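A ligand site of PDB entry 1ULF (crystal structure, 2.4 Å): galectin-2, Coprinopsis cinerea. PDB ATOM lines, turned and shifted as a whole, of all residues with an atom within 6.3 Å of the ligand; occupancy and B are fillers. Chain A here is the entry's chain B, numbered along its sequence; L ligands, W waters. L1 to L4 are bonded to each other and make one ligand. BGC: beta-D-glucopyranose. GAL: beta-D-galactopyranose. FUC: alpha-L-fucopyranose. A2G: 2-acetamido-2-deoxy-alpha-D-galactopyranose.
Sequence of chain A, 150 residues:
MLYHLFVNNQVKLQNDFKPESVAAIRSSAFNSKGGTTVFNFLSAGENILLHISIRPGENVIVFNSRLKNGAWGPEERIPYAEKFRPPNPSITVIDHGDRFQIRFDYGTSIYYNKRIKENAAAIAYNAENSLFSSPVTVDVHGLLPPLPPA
Water W6 lies within hydrogen-bond range of O4 of GAL L2 (2.6 Å) and OG of Ser 53 (2.8 Å).
Water W2 lies within hydrogen-bond range of an oxygen (O7) of A2G L4 (2.8 Å) and the side-chain amide nitrogen of Asn 40 (2.9 Å).
Water W3 bridges NH2 of Arg 66 and O4 of A2G L4.
The guanidinium group (NH1) of Arg 77 is in salt-bridge range of the side-chain carboxylate (OE2) of Glu 58 (2.7 Å).
The backbone carbonyl oxygen of Asn 126 lies within hydrogen-bond range of the backbone NH of Val 38 (2.7 Å).
The backbone NH of His 51 sits at hydrogen-bond distance from the backbone carbonyl oxygen of Asn 64, 2.8 Å away.
NH2 of Arg 55 lies within salt-bridge range of OE2 of Glu 75, 3.998 Å away.
OD1 of Asn 40 lies within hydrogen-bond range of ND1 of His 51.
The backbone carbonyl oxygen of Val 62 is in hydrogen-bond range of the backbone NH of Ser 53, 2.8 Å away.
The guanidinium group (NH1) of Arg 66 is in hydrogen-bond range of the backbone carbonyl oxygen (O) of Gly 70 (2.9 Å).
The side-chain amide oxygen (OD1) of Asn 64 lies close to the backbone carbonyl oxygen (O) of Pro 74, at 3.4 Å.
A ring nitrogen (NE2) of His 51 lies within hydrogen-bond range of an oxygen (O4) of GAL L2 (2.8 Å).
An oxygen (O6) of GAL L2 sits at hydrogen-bond distance from the side-chain amide nitrogen (ND2) of Asn 64.
The guanidinium group (NH1) of Arg 55 lies within hydrogen-bond range of an oxygen (O3) of BGC L1, at 2.8 Å.
NH2 of Arg 77 sits at hydrogen-bond distance from O3 of BGC L1 (3.5 Å).
NE1 of Trp 72 is in hydrogen-bond range of O6 of A2G L4 (3.0 Å).
O3 of BGC L1 sits at hydrogen-bond distance from OE2 of Glu 75, 2.5 Å away.
Merely in contact with the ligand: Val 38, Val 62, Arg 66 and Asn 126.
Hydrophobic or aromatic side chains that line the ligand: Val 38, His 51, Val 62 and Trp 72.
Within 4 Å of the ligand: Val 38, His 51, Arg 55, Val 62, Asn 64, Arg 66, Trp 72, Glu 75, Arg 77 and Asn 126.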
ATOM      1  N   THR A  36      15.138   4.283  16.304  1.00  0.00           N
ATOM      2  CA  THR A  36      15.095   3.309  15.223  1.00  0.00           C
ATOM      3  C   THR A  36      13.934   2.324  15.418  1.00  0.00           C
ATOM      4  O   THR A  36      13.808   1.684  16.460  1.00  0.00           O
ATOM      5  CB  THR A  36      16.453   2.553  15.116  1.00  0.00           C
ATOM      6  OG1 THR A  36      17.434   3.451  14.580  1.00  0.00           O
ATOM      7  CG2 THR A  36      16.353   1.338  14.217  1.00  0.00           C
ATOM      8  N   THR A  37      13.097   2.244  14.392  1.00  0.00           N
ATOM      9  CA  THR A  37      11.915   1.382  14.401  1.00  0.00           C
ATOM     10  C   THR A  37      12.016   0.387  13.233  1.00  0.00           C
ATOM     11  O   THR A  37      12.179   0.790  12.080  1.00  0.00           O
ATOM     12  CB  THR A  37      10.642   2.227  14.248  1.00  0.00           C
ATOM     13  OG1 THR A  37      10.649   3.254  15.256  1.00  0.00           O
ATOM     14  CG2 THR A  37       9.397   1.378  14.409  1.00  0.00           C
ATOM     15  N   VAL A  38      11.887  -0.893  13.538  1.00  0.00           N
ATOM     16  CA  VAL A  38      12.023  -1.929  12.523  1.00  0.00           C
ATOM     17  C   VAL A  38      10.819  -2.816  12.283  1.00  0.00           C
ATOM     18  O   VAL A  38      10.020  -3.070  13.183  1.00  0.00           O
ATOM     19  CB  VAL A  38      13.210  -2.851  12.873  1.00  0.00           C
ATOM     20  CG1 VAL A  38      13.219  -4.079  11.981  1.00  0.00           C
ATOM     21  CG2 VAL A  38      14.514  -2.079  12.737  1.00  0.00           C
ATOM     22  N   ASN A  40      10.082  -6.537  10.117  1.00  0.00           N
ATOM     23  CA  ASN A  40      10.675  -7.647   9.392  1.00  0.00           C
ATOM     24  C   ASN A  40       9.620  -8.616   8.882  1.00  0.00           C
ATOM     25  O   ASN A  40       8.620  -8.867   9.546  1.00  0.00           O
ATOM     26  CB  ASN A  40      11.619  -8.467  10.287  1.00  0.00           C
ATOM     27  CG  ASN A  40      12.831  -7.698  10.753  1.00  0.00           C
ATOM     28  OD1 ASN A  40      13.420  -6.931   9.998  1.00  0.00           O
ATOM     29  ND2 ASN A  40      13.225  -7.912  12.002  1.00  0.00           N
ATOM     30  N   HIS A  51      13.782  -6.649   5.602  1.00  0.00           N
ATOM     31  CA  HIS A  51      14.063  -5.905   6.820  1.00  0.00           C
ATOM     32  C   HIS A  51      13.934  -4.406   6.494  1.00  0.00           C
ATOM     33  O   HIS A  51      14.562  -3.923   5.561  1.00  0.00           O
ATOM     34  CB  HIS A  51      15.489  -6.239   7.276  1.00  0.00           C
ATOM     35  CG  HIS A  51      15.978  -5.414   8.424  1.00  0.00           C
ATOM     36  ND1 HIS A  51      15.512  -5.562   9.717  1.00  0.00           N
ATOM     37  CD2 HIS A  51      16.944  -4.469   8.491  1.00  0.00           C
ATOM     38  CE1 HIS A  51      16.169  -4.751  10.514  1.00  0.00           C
ATOM     39  NE2 HIS A  51      17.046  -4.071   9.796  1.00  0.00           N
ATOM     40  N   SER A  53      14.507  -0.928   8.344  1.00  0.00           N
ATOM     41  CA  SER A  53      15.014  -0.238   9.521  1.00  0.00           C
ATOM     42  C   SER A  53      14.883   1.275   9.365  1.00  0.00           C
ATOM     43  O   SER A  53      15.682   1.906   8.669  1.00  0.00           O
ATOM     44  CB  SER A  53      16.488  -0.622   9.746  1.00  0.00           C
ATOM     45  OG  SER A  53      17.051   0.128  10.803  1.00  0.00           O
ATOM     46  N   ARG A  55      15.500   4.724  10.581  1.00  0.00           N
ATOM     47  CA  ARG A  55      16.421   5.405  11.483  1.00  0.00           C
ATOM     48  C   ARG A  55      16.367   6.922  11.373  1.00  0.00           C
ATOM     49  O   ARG A  55      17.019   7.517  10.510  1.00  0.00           O
ATOM     50  CB  ARG A  55      17.843   4.919  11.199  1.00  0.00           C
ATOM     51  CG  ARG A  55      17.976   3.404  11.198  1.00  0.00           C
ATOM     52  CD  ARG A  55      19.382   2.961  10.797  1.00  0.00           C
ATOM     53  NE  ARG A  55      19.440   1.508  10.664  1.00  0.00           N
ATOM     54  CZ  ARG A  55      20.530   0.837  10.302  1.00  0.00           C
ATOM     55  NH1 ARG A  55      21.652   1.491  10.040  1.00  0.00           N
ATOM     56  NH2 ARG A  55      20.483  -0.490  10.197  1.00  0.00           N
ATOM     57  N   GLU A  58      19.741   8.753  11.904  1.00  0.00           N
ATOM     58  CA  GLU A  58      20.714   8.606  10.820  1.00  0.00           C
ATOM     59  C   GLU A  58      20.100   9.165   9.541  1.00  0.00           C
ATOM     60  O   GLU A  58      20.746   9.195   8.489  1.00  0.00           O
ATOM     61  CB  GLU A  58      21.037   7.123  10.647  1.00  0.00           C
ATOM     62  CG  GLU A  58      22.419   6.816  10.087  1.00  0.00           C
ATOM     63  CD  GLU A  58      22.674   5.314   9.949  1.00  0.00           C
ATOM     64  OE1 GLU A  58      22.447   4.558  10.920  1.00  0.00           O
ATOM     65  OE2 GLU A  58      23.106   4.879   8.853  1.00  0.00           O
ATOM     66  N   VAL A  62      16.775   1.829   6.034  1.00  0.00           N
ATOM     67  CA  VAL A  62      17.592   0.748   5.509  1.00  0.00           C
ATOM     68  C   VAL A  62      16.827  -0.524   5.165  1.00  0.00           C
ATOM     69  O   VAL A  62      16.083  -1.047   5.994  1.00  0.00           O
ATOM     70  CB  VAL A  62      18.715   0.378   6.516  1.00  0.00           C
ATOM     71  CG1 VAL A  62      19.547  -0.769   5.970  1.00  0.00           C
ATOM     72  CG2 VAL A  62      19.574   1.598   6.809  1.00  0.00           C
ATOM     73  N   PHE A  63      17.035  -1.021   3.950  1.00  0.00           N
ATOM     74  CA  PHE A  63      16.394  -2.246   3.508  1.00  0.00           C
ATOM     75  C   PHE A  63      17.449  -3.340   3.367  1.00  0.00           C
ATOM     76  O   PHE A  63      18.523  -3.117   2.798  1.00  0.00           O
ATOM     77  CB  PHE A  63      15.682  -2.043   2.170  1.00  0.00           C
ATOM     78  CG  PHE A  63      14.536  -1.083   2.232  1.00  0.00           C
ATOM     79  CD1 PHE A  63      14.761   0.284   2.205  1.00  0.00           C
ATOM     80  CD2 PHE A  63      13.230  -1.549   2.336  1.00  0.00           C
ATOM     81  CE1 PHE A  63      13.693   1.190   2.277  1.00  0.00           C
ATOM     82  CE2 PHE A  63      12.153  -0.660   2.409  1.00  0.00           C
ATOM     83  CZ  PHE A  63      12.390   0.712   2.377  1.00  0.00           C
ATOM     84  N   ASN A  64      17.140  -4.521   3.891  1.00  0.00           N
ATOM     85  CA  ASN A  64      18.096  -5.617   3.825  1.00  0.00           C
ATOM     86  C   ASN A  64      17.439  -6.965   4.060  1.00  0.00           C
ATOM     87  O   ASN A  64      16.226  -7.059   4.240  1.00  0.00           O
ATOM     88  CB  ASN A  64      19.205  -5.400   4.867  1.00  0.00           C
ATOM     89  CG  ASN A  64      20.541  -5.920   4.412  1.00  0.00           C
ATOM     90  OD1 ASN A  64      20.624  -6.756   3.518  1.00  0.00           O
ATOM     91  ND2 ASN A  64      21.616  -5.427   5.019  1.00  0.00           N
ATOM     92  N   ARG A  66      18.598 -11.364   5.387  1.00  0.00           N
ATOM     93  CA  ARG A  66      19.591 -12.270   5.944  1.00  0.00           C
ATOM     94  C   ARG A  66      18.932 -13.524   6.478  1.00  0.00           C
ATOM     95  O   ARG A  66      17.793 -13.485   6.943  1.00  0.00           O
ATOM     96  CB  ARG A  66      20.405 -11.598   7.055  1.00  0.00           C
ATOM     97  CG  ARG A  66      19.688 -11.428   8.379  1.00  0.00           C
ATOM     98  CD  ARG A  66      20.707 -11.298   9.506  1.00  0.00           C
ATOM     99  NE  ARG A  66      20.099 -11.040  10.803  1.00  0.00           N
ATOM    100  CZ  ARG A  66      20.615 -11.456  11.967  1.00  0.00           C
ATOM    101  NH1 ARG A  66      21.737 -12.164  11.982  1.00  0.00           N
ATOM    102  NH2 ARG A  66      20.009 -11.154  13.107  1.00  0.00           N
ATOM    103  N   GLY A  70      22.315 -15.355   9.966  1.00  0.00           N
ATOM    104  CA  GLY A  70      23.329 -15.092   8.966  1.00  0.00           C
ATOM    105  C   GLY A  70      23.809 -13.658   8.901  1.00  0.00           C
ATOM    106  O   GLY A  70      23.492 -12.833   9.769  1.00  0.00           O
ATOM    107  N   TRP A  72      24.089  -9.915   7.190  1.00  0.00           N
ATOM    108  CA  TRP A  72      23.240  -8.997   6.442  1.00  0.00           C
ATOM    109  C   TRP A  72      23.891  -8.802   5.071  1.00  0.00           C
ATOM    110  O   TRP A  72      25.120  -8.875   4.948  1.00  0.00           O
ATOM    111  CB  TRP A  72      23.148  -7.657   7.162  1.00  0.00           C
ATOM    112  CG  TRP A  72      22.292  -7.674   8.393  1.00  0.00           C
ATOM    113  CD1 TRP A  72      22.726  -7.659   9.697  1.00  0.00           C
ATOM    114  CD2 TRP A  72      20.863  -7.709   8.444  1.00  0.00           C
ATOM    115  NE1 TRP A  72      21.651  -7.675  10.544  1.00  0.00           N
ATOM    116  CE2 TRP A  72      20.493  -7.715   9.816  1.00  0.00           C
ATOM    117  CE3 TRP A  72      19.860  -7.755   7.473  1.00  0.00           C
ATOM    118  CZ2 TRP A  72      19.162  -7.743  10.227  1.00  0.00           C
ATOM    119  CZ3 TRP A  72      18.529  -7.784   7.883  1.00  0.00           C
ATOM    120  CH2 TRP A  72      18.193  -7.773   9.255  1.00  0.00           C
ATOM    121  N   GLY A  73      23.073  -8.573   4.049  1.00  0.00           N
ATOM    122  CA  GLY A  73      23.601  -8.358   2.711  1.00  0.00           C
ATOM    123  C   GLY A  73      23.842  -6.876   2.481  1.00  0.00           C
ATOM    124  O   GLY A  73      23.824  -6.086   3.425  1.00  0.00           O
ATOM    125  N   PRO A  74      24.098  -6.456   1.226  1.00  0.00           N
ATOM    126  CA  PRO A  74      24.319  -5.009   1.018  1.00  0.00           C
ATOM    127  C   PRO A  74      23.048  -4.240   1.367  1.00  0.00           C
ATOM    128  O   PRO A  74      21.938  -4.700   1.080  1.00  0.00           O
ATOM    129  CB  PRO A  74      24.685  -4.923  -0.468  1.00  0.00           C
ATOM    130  CG  PRO A  74      24.083  -6.170  -1.074  1.00  0.00           C
ATOM    131  CD  PRO A  74      24.311  -7.217  -0.016  1.00  0.00           C
ATOM    132  N   GLU A  75      23.218  -3.088   2.013  1.00  0.00           N
ATOM    133  CA  GLU A  75      22.071  -2.284   2.417  1.00  0.00           C
ATOM    134  C   GLU A  75      21.579  -1.391   1.282  1.00  0.00           C
ATOM    135  O   GLU A  75      22.362  -0.820   0.524  1.00  0.00           O
ATOM    136  CB  GLU A  75      22.438  -1.382   3.611  1.00  0.00           C
ATOM    137  CG  GLU A  75      23.031  -2.078   4.826  1.00  0.00           C
ATOM    138  CD  GLU A  75      23.167  -1.142   6.025  1.00  0.00           C
ATOM    139  OE1 GLU A  75      23.588   0.027   5.838  1.00  0.00           O
ATOM    140  OE2 GLU A  75      22.863  -1.560   7.168  1.00  0.00           O
ATOM    141  N   ARG A  77      19.454   1.843   0.925  1.00  0.00           N
ATOM    142  CA  ARG A  77      18.860   2.897   1.705  1.00  0.00           C
ATOM    143  C   ARG A  77      18.374   4.119   0.949  1.00  0.00           C
ATOM    144  O   ARG A  77      18.754   4.360  -0.199  1.00  0.00           O
ATOM    145  CB  ARG A  77      19.815   3.322   2.835  1.00  0.00           C
ATOM    146  CG  ARG A  77      21.279   3.382   2.453  1.00  0.00           C
ATOM    147  CD  ARG A  77      22.105   3.991   3.579  1.00  0.00           C
ATOM    148  NE  ARG A  77      22.562   3.025   4.580  1.00  0.00           N
ATOM    149  CZ  ARG A  77      23.038   3.357   5.781  1.00  0.00           C
ATOM    150  NH1 ARG A  77      23.103   4.643   6.124  1.00  0.00           N
ATOM    151  NH2 ARG A  77      23.451   2.436   6.634  1.00  0.00           N
ATOM    152  N   ASN A 126       9.945  -4.248  15.723  1.00  0.00           N
ATOM    153  CA  ASN A 126      10.942  -3.994  16.776  1.00  0.00           C
ATOM    154  C   ASN A 126      11.248  -2.521  16.981  1.00  0.00           C
ATOM    155  O   ASN A 126      11.357  -1.758  16.018  1.00  0.00           O
ATOM    156  CB  ASN A 126      12.261  -4.708  16.463  1.00  0.00           C
ATOM    157  CG  ASN A 126      12.137  -6.220  16.472  1.00  0.00           C
ATOM    158  OD1 ASN A 126      11.486  -6.794  17.339  1.00  0.00           O
ATOM    159  ND2 ASN A 126      12.775  -6.868  15.508  1.00  0.00           N
ATOM    160  N   ALA A 127      11.384  -2.130  18.238  1.00  0.00           N
ATOM    161  CA  ALA A 127      11.723  -0.753  18.575  1.00  0.00           C
ATOM    162  C   ALA A 127      11.837  -0.598  20.077  1.00  0.00           C
ATOM    163  O   ALA A 127      11.053  -1.169  20.835  1.00  0.00           O
ATOM    164  CB  ALA A 127      10.656   0.205  18.038  1.00  0.00           C
HETATM  165  C2  BGC L   1      26.126  -0.113   9.023  1.00  0.00           C
HETATM  166  C3  BGC L   1      24.855  -0.353   9.826  1.00  0.00           C
HETATM  167  C4  BGC L   1      24.806  -1.787  10.363  1.00  0.00           C
HETATM  168  C5  BGC L   1      26.112  -2.123  11.112  1.00  0.00           C
HETATM  169  C6  BGC L   1      26.227  -3.568  11.544  1.00  0.00           C
HETATM  170  C1  BGC L   1      27.319  -0.454   9.918  1.00  0.00           C
HETATM  171  O1  BGC L   1      28.496  -0.243   9.226  1.00  0.00           O
HETATM  172  O2  BGC L   1      26.201   1.252   8.626  1.00  0.00           O
HETATM  173  O3  BGC L   1      23.708  -0.092   9.027  1.00  0.00           O
HETATM  174  O4  BGC L   1      23.681  -1.901  11.265  1.00  0.00           O
HETATM  175  O5  BGC L   1      27.256  -1.837  10.284  1.00  0.00           O
HETATM  176  O6  BGC L   1      25.911  -4.463  10.485  1.00  0.00           O
HETATM  177  C1  GAL L   2      22.905  -3.051  11.173  1.00  0.00           C
HETATM  178  C2  GAL L   2      22.038  -3.164  12.433  1.00  0.00           C
HETATM  179  C3  GAL L   2      21.060  -4.342  12.298  1.00  0.00           C
HETATM  180  C4  GAL L   2      20.280  -4.272  10.970  1.00  0.00           C
HETATM  181  C5  GAL L   2      21.267  -4.132   9.811  1.00  0.00           C
HETATM  182  C6  GAL L   2      20.593  -4.018   8.471  1.00  0.00           C
HETATM  183  O2  GAL L   2      22.884  -3.373  13.580  1.00  0.00           O
HETATM  184  O3  GAL L   2      20.147  -4.317  13.407  1.00  0.00           O
HETATM  185  O4  GAL L   2      19.378  -3.172  10.993  1.00  0.00           O
HETATM  186  O5  GAL L   2      22.084  -2.958  10.001  1.00  0.00           O
HETATM  187  O6  GAL L   2      21.557  -3.773   7.443  1.00  0.00           O
HETATM  188  C1  FUC L   3      22.470  -2.787  14.790  1.00  0.00           C
HETATM  189  C2  FUC L   3      23.497  -3.106  15.871  1.00  0.00           C
HETATM  190  C3  FUC L   3      24.818  -2.366  15.588  1.00  0.00           C
HETATM  191  C4  FUC L   3      24.593  -0.872  15.324  1.00  0.00           C
HETATM  192  C5  FUC L   3      23.475  -0.663  14.302  1.00  0.00           C
HETATM  193  C6  FUC L   3      23.073   0.791  14.147  1.00  0.00           C
HETATM  194  O2  FUC L   3      23.745  -4.500  15.915  1.00  0.00           O
HETATM  195  O3  FUC L   3      25.692  -2.534  16.700  1.00  0.00           O
HETATM  196  O4  FUC L   3      24.271  -0.211  16.534  1.00  0.00           O
HETATM  197  O5  FUC L   3      22.285  -1.382  14.689  1.00  0.00           O
HETATM  198  O5  A2G L   4      20.119  -6.653  13.560  1.00  0.00           O
HETATM  199  C1  A2G L   4      19.343  -5.462  13.539  1.00  0.00           C
HETATM  200  C2  A2G L   4      18.485  -5.341  14.790  1.00  0.00           C
HETATM  201  N2  A2G L   4      17.823  -4.052  14.809  1.00  0.00           N
HETATM  202  C3  A2G L   4      19.349  -5.502  16.062  1.00  0.00           C
HETATM  203  O3  A2G L   4      18.500  -5.557  17.205  1.00  0.00           O
HETATM  204  C4  A2G L   4      20.197  -6.779  15.979  1.00  0.00           C
HETATM  205  O4  A2G L   4      19.343  -7.920  15.967  1.00  0.00           O
HETATM  206  C5  A2G L   4      21.019  -6.744  14.689  1.00  0.00           C
HETATM  207  C6  A2G L   4      21.895  -7.956  14.475  1.00  0.00           C
HETATM  208  O6  A2G L   4      22.716  -7.784  13.326  1.00  0.00           O
HETATM  209  C7  A2G L   4      16.522  -3.984  15.061  1.00  0.00           C
HETATM  210  O7  A2G L   4      15.719  -4.804  14.633  1.00  0.00           O
HETATM  211  C8  A2G L   4      16.037  -2.830  15.917  1.00  0.00           C
HETATM  212  O   HOH W   1      19.715  -0.212  14.444  1.00  0.00           O
HETATM  213  O   HOH W   2      15.810  -7.026  12.934  1.00  0.00           O
HETATM  214  O   HOH W   3      17.803  -9.063  13.520  1.00  0.00           O
HETATM  215  O   HOH W   4      19.625  -1.988  16.627  1.00  0.00           O
HETATM  216  O   HOH W   5      25.481   2.002  16.919  1.00  0.00           O
HETATM  217  O   HOH W   6      18.088  -1.667  12.663  1.00  0.00           O
HETATM  218  O   HOH W   7      22.730  -5.595  18.006  1.00  0.00           O
